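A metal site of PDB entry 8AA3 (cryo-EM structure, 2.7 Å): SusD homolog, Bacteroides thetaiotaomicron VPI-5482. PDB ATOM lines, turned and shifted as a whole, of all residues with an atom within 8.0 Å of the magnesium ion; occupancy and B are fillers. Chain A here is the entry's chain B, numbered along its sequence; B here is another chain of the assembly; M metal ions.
The side-chain amide oxygen (OD1) of Asn 281 is in hydrogen-bond range of the side-chain amide nitrogen (ND2) of Asn 419.
The side-chain carboxylate (OD2) of Asp 684 of chain B is in hydrogen-bond range of the backbone NH (N) of Asn 689 of chain B, 2.7 Å away.
The side-chain amide oxygen of Asn 419 sits close to the backbone carbonyl oxygen of Ile 289 (3.4 Å).
OE1 of Gln 290 sits at hydrogen-bond distance from ND2 of Asn 419 (3.2 Å).
The nearest printed residue that does not touch the magnesium ion is Gln 290 (4.4 Å).
OD1 of Asn 419 binds the magnesium ion (2.1 Å).
The magnesium ion is bound by the backbone carbonyl oxygen (O) of Tyr 291 (2.1 Å).
ND2 of Asn 689 of chain B is bound to the magnesium ion.
The magnesium ion is bound by OE1 of Glu 280, 2.4 Å away.
The magnesium ion is bound by O of Ser 417 (2.6 Å).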
ATOM      1  N   PRO A 277     -29.361  18.653  21.262  1.00  0.00           N
ATOM      2  CA  PRO A 277     -29.293  17.245  21.692  1.00  0.00           C
ATOM      3  C   PRO A 277     -30.549  16.760  22.399  1.00  0.00           C
ATOM      4  O   PRO A 277     -30.869  15.566  22.321  1.00  0.00           O
ATOM      5  CB  PRO A 277     -28.078  17.227  22.636  1.00  0.00           C
ATOM      6  CG  PRO A 277     -27.258  18.413  22.225  1.00  0.00           C
ATOM      7  CD  PRO A 277     -28.249  19.453  21.810  1.00  0.00           C
ATOM      8  N   GLU A 280     -33.218  15.148  19.762  1.00  0.00           N
ATOM      9  CA  GLU A 280     -32.676  14.327  18.682  1.00  0.00           C
ATOM     10  C   GLU A 280     -33.746  13.384  18.146  1.00  0.00           C
ATOM     11  O   GLU A 280     -34.638  12.947  18.866  1.00  0.00           O
ATOM     12  CB  GLU A 280     -31.464  13.534  19.176  1.00  0.00           C
ATOM     13  CG  GLU A 280     -30.153  14.281  19.092  1.00  0.00           C
ATOM     14  CD  GLU A 280     -28.948  13.378  19.302  1.00  0.00           C
ATOM     15  OE1 GLU A 280     -29.088  12.159  19.114  1.00  0.00           O
ATOM     16  OE2 GLU A 280     -27.869  13.899  19.652  1.00  0.00           O
ATOM     17  N   ASN A 281     -33.632  13.073  16.851  1.00  0.00           N
ATOM     18  CA  ASN A 281     -34.567  12.193  16.155  1.00  0.00           C
ATOM     19  C   ASN A 281     -36.001  12.702  16.273  1.00  0.00           C
ATOM     20  O   ASN A 281     -36.920  11.966  16.655  1.00  0.00           O
ATOM     21  CB  ASN A 281     -34.451  10.749  16.661  1.00  0.00           C
ATOM     22  CG  ASN A 281     -33.074  10.156  16.433  1.00  0.00           C
ATOM     23  OD1 ASN A 281     -32.383  10.521  15.478  1.00  0.00           O
ATOM     24  ND2 ASN A 281     -32.670   9.245  17.295  1.00  0.00           N
ATOM     25  N   ALA A 288     -31.086  10.866   9.869  1.00  0.00           N
ATOM     26  CA  ALA A 288     -29.918  11.503  10.462  1.00  0.00           C
ATOM     27  C   ALA A 288     -28.879  10.443  10.806  1.00  0.00           C
ATOM     28  O   ALA A 288     -29.194   9.258  10.973  1.00  0.00           O
ATOM     29  CB  ALA A 288     -30.293  12.295  11.722  1.00  0.00           C
ATOM     30  N   ILE A 289     -27.627  10.888  10.893  1.00  0.00           N
ATOM     31  CA  ILE A 289     -26.535  10.020  11.320  1.00  0.00           C
ATOM     32  C   ILE A 289     -26.500  10.004  12.838  1.00  0.00           C
ATOM     33  O   ILE A 289     -26.317  11.043  13.480  1.00  0.00           O
ATOM     34  CB  ILE A 289     -25.193  10.486  10.735  1.00  0.00           C
ATOM     35  CG1 ILE A 289     -25.261  10.550   9.208  1.00  0.00           C
ATOM     36  CG2 ILE A 289     -24.067   9.573  11.181  1.00  0.00           C
ATOM     37  CD1 ILE A 289     -25.791   9.287   8.564  1.00  0.00           C
ATOM     38  N   GLN A 290     -26.666   8.817  13.418  1.00  0.00           N
ATOM     39  CA  GLN A 290     -26.764   8.675  14.873  1.00  0.00           C
ATOM     40  C   GLN A 290     -25.371   8.729  15.477  1.00  0.00           C
ATOM     41  O   GLN A 290     -24.591   7.786  15.348  1.00  0.00           O
ATOM     42  CB  GLN A 290     -27.479   7.379  15.231  1.00  0.00           C
ATOM     43  CG  GLN A 290     -28.757   7.130  14.449  1.00  0.00           C
ATOM     44  CD  GLN A 290     -29.784   8.214  14.665  1.00  0.00           C
ATOM     45  OE1 GLN A 290     -30.415   8.296  15.725  1.00  0.00           O
ATOM     46  NE2 GLN A 290     -29.970   9.062  13.659  1.00  0.00           N
ATOM     47  N   TYR A 291     -25.066   9.843  16.143  1.00  0.00           N
ATOM     48  CA  TYR A 291     -23.804  10.004  16.866  1.00  0.00           C
ATOM     49  C   TYR A 291     -24.047   9.745  18.350  1.00  0.00           C
ATOM     50  O   TYR A 291     -25.010  10.260  18.927  1.00  0.00           O
ATOM     51  CB  TYR A 291     -23.232  11.409  16.657  1.00  0.00           C
ATOM     52  CG  TYR A 291     -22.714  11.650  15.249  1.00  0.00           C
ATOM     53  CD1 TYR A 291     -21.547  11.040  14.804  1.00  0.00           C
ATOM     54  CD2 TYR A 291     -23.397  12.485  14.376  1.00  0.00           C
ATOM     55  CE1 TYR A 291     -21.077  11.258  13.519  1.00  0.00           C
ATOM     56  CE2 TYR A 291     -22.936  12.707  13.090  1.00  0.00           C
ATOM     57  CZ  TYR A 291     -21.771  12.095  12.676  1.00  0.00           C
ATOM     58  OH  TYR A 291     -21.301  12.313  11.391  1.00  0.00           O
ATOM     59  N   SER A 292     -23.188   8.935  18.957  1.00  0.00           N
ATOM     60  CA  SER A 292     -23.388   8.474  20.322  1.00  0.00           C
ATOM     61  C   SER A 292     -22.159   8.765  21.170  1.00  0.00           C
ATOM     62  O   SER A 292     -21.043   8.917  20.667  1.00  0.00           O
ATOM     63  CB  SER A 292     -23.690   6.972  20.358  1.00  0.00           C
ATOM     64  OG  SER A 292     -22.797   6.240  19.540  1.00  0.00           O
ATOM     65  N   ILE A 293     -22.389   8.850  22.477  1.00  0.00           N
ATOM     66  CA  ILE A 293     -21.336   9.058  23.461  1.00  0.00           C
ATOM     67  C   ILE A 293     -21.481   8.004  24.553  1.00  0.00           C
ATOM     68  O   ILE A 293     -22.568   7.464  24.777  1.00  0.00           O
ATOM     69  CB  ILE A 293     -21.400  10.488  24.058  1.00  0.00           C
ATOM     70  CG1 ILE A 293     -20.080  10.844  24.760  1.00  0.00           C
ATOM     71  CG2 ILE A 293     -22.570  10.635  25.008  1.00  0.00           C
ATOM     72  CD1 ILE A 293     -19.727  12.311  24.686  1.00  0.00           C
ATOM     73  N   ASN A 301     -18.746   7.627  19.342  1.00  0.00           N
ATOM     74  CA  ASN A 301     -18.952   7.900  17.919  1.00  0.00           C
ATOM     75  C   ASN A 301     -19.444   9.345  17.760  1.00  0.00           C
ATOM     76  O   ASN A 301     -20.582   9.620  17.377  1.00  0.00           O
ATOM     77  CB  ASN A 301     -19.919   6.909  17.304  1.00  0.00           C
ATOM     78  CG  ASN A 301     -19.401   5.487  17.342  1.00  0.00           C
ATOM     79  OD1 ASN A 301     -20.110   4.562  17.733  1.00  0.00           O
ATOM     80  ND2 ASN A 301     -18.147   5.304  16.941  1.00  0.00           N
ATOM     81  N   SER A 416     -19.050  16.504  19.501  1.00  0.00           N
ATOM     82  CA  SER A 416     -20.245  16.179  20.268  1.00  0.00           C
ATOM     83  C   SER A 416     -20.974  15.011  19.627  1.00  0.00           C
ATOM     84  O   SER A 416     -20.587  14.500  18.576  1.00  0.00           O
ATOM     85  CB  SER A 416     -21.157  17.408  20.379  1.00  0.00           C
ATOM     86  OG  SER A 416     -21.684  17.760  19.105  1.00  0.00           O
ATOM     87  N   SER A 417     -22.065  14.591  20.275  1.00  0.00           N
ATOM     88  CA  SER A 417     -22.884  13.478  19.802  1.00  0.00           C
ATOM     89  C   SER A 417     -24.149  13.953  19.101  1.00  0.00           C
ATOM     90  O   SER A 417     -25.057  13.144  18.870  1.00  0.00           O
ATOM     91  CB  SER A 417     -23.245  12.560  20.970  1.00  0.00           C
ATOM     92  OG  SER A 417     -24.023  13.244  21.936  1.00  0.00           O
ATOM     93  N   LEU A 418     -24.236  15.234  18.755  1.00  0.00           N
ATOM     94  CA  LEU A 418     -25.415  15.751  18.068  1.00  0.00           C
ATOM     95  C   LEU A 418     -25.558  15.096  16.701  1.00  0.00           C
ATOM     96  O   LEU A 418     -24.594  14.997  15.940  1.00  0.00           O
ATOM     97  CB  LEU A 418     -25.319  17.276  17.928  1.00  0.00           C
ATOM     98  CG  LEU A 418     -26.503  17.975  17.270  1.00  0.00           C
ATOM     99  CD1 LEU A 418     -27.766  17.794  18.111  1.00  0.00           C
ATOM    100  CD2 LEU A 418     -26.219  19.448  17.056  1.00  0.00           C
ATOM    101  N   ASN A 419     -26.774  14.663  16.392  1.00  0.00           N
ATOM    102  CA  ASN A 419     -27.025  13.975  15.133  1.00  0.00           C
ATOM    103  C   ASN A 419     -26.988  14.956  13.964  1.00  0.00           C
ATOM    104  O   ASN A 419     -27.459  16.087  14.065  1.00  0.00           O
ATOM    105  CB  ASN A 419     -28.375  13.257  15.172  1.00  0.00           C
ATOM    106  CG  ASN A 419     -28.350  12.028  16.046  1.00  0.00           C
ATOM    107  OD1 ASN A 419     -27.340  11.712  16.676  1.00  0.00           O
ATOM    108  ND2 ASN A 419     -29.475  11.320  16.096  1.00  0.00           N
ATOM    109  N   HIS A 420     -26.419  14.500  12.845  1.00  0.00           N
ATOM    110  CA  HIS A 420     -26.384  15.281  11.611  1.00  0.00           C
ATOM    111  C   HIS A 420     -27.585  14.886  10.765  1.00  0.00           C
ATOM    112  O   HIS A 420     -27.617  13.774  10.202  1.00  0.00           O
ATOM    113  CB  HIS A 420     -25.072  15.055  10.865  1.00  0.00           C
ATOM    114  CG  HIS A 420     -25.035  15.688   9.512  1.00  0.00           C
ATOM    115  ND1 HIS A 420     -24.936  17.051   9.328  1.00  0.00           N
ATOM    116  CD2 HIS A 420     -25.089  15.139   8.267  1.00  0.00           C
ATOM    117  CE1 HIS A 420     -24.925  17.325   8.033  1.00  0.00           C
ATOM    118  NE2 HIS A 420     -25.014  16.177   7.369  1.00  0.00           N
ATOM    119  N   ASP B 684     -24.955   3.397  16.554  1.00  0.00           N
ATOM    120  CA  ASP B 684     -26.124   3.445  17.436  1.00  0.00           C
ATOM    121  C   ASP B 684     -27.373   3.371  16.557  1.00  0.00           C
ATOM    122  O   ASP B 684     -28.035   4.368  16.262  1.00  0.00           O
ATOM    123  CB  ASP B 684     -26.099   4.708  18.283  1.00  0.00           C
ATOM    124  CG  ASP B 684     -27.191   4.722  19.342  1.00  0.00           C
ATOM    125  OD1 ASP B 684     -27.832   3.668  19.543  1.00  0.00           O
ATOM    126  OD2 ASP B 684     -27.409   5.777  19.969  1.00  0.00           O
ATOM    127  N   GLY B 687     -30.519   4.711  18.212  1.00  0.00           N
ATOM    128  CA  GLY B 687     -30.590   6.159  18.331  1.00  0.00           C
ATOM    129  C   GLY B 687     -30.794   6.620  19.761  1.00  0.00           C
ATOM    130  O   GLY B 687     -31.529   7.575  20.008  1.00  0.00           O
ATOM    131  N   SER B 688     -30.139   5.943  20.702  1.00  0.00           N
ATOM    132  CA  SER B 688     -30.252   6.265  22.118  1.00  0.00           C
ATOM    133  C   SER B 688     -29.061   7.066  22.638  1.00  0.00           C
ATOM    134  O   SER B 688     -28.909   7.206  23.852  1.00  0.00           O
ATOM    135  CB  SER B 688     -30.415   4.984  22.936  1.00  0.00           C
ATOM    136  OG  SER B 688     -29.314   4.108  22.736  1.00  0.00           O
ATOM    137  N   ASN B 689     -28.220   7.593  21.745  1.00  0.00           N
ATOM    138  CA  ASN B 689     -27.035   8.367  22.118  1.00  0.00           C
ATOM    139  C   ASN B 689     -26.116   7.570  23.037  1.00  0.00           C
ATOM    140  O   ASN B 689     -25.593   8.088  24.028  1.00  0.00           O
ATOM    141  CB  ASN B 689     -27.422   9.701  22.763  1.00  0.00           C
ATOM    142  CG  ASN B 689     -28.022  10.679  21.766  1.00  0.00           C
ATOM    143  OD1 ASN B 689     -29.196  11.032  21.851  1.00  0.00           O
ATOM    144  ND2 ASN B 689     -27.211  11.111  20.805  1.00  0.00           N
ATOM    145  N   GLY B 690     -25.916   6.289  22.714  1.00  0.00           N
ATOM    146  CA  GLY B 690     -25.031   5.456  23.489  1.00  0.00           C
ATOM    147  C   GLY B 690     -25.689   4.949  24.766  1.00  0.00           C
ATOM    148  O   GLY B 690     -26.901   4.771  24.849  1.00  0.00           O
HETATM  149 MG    MG M   1     -26.863  11.309  18.668  1.00  0.00          MG
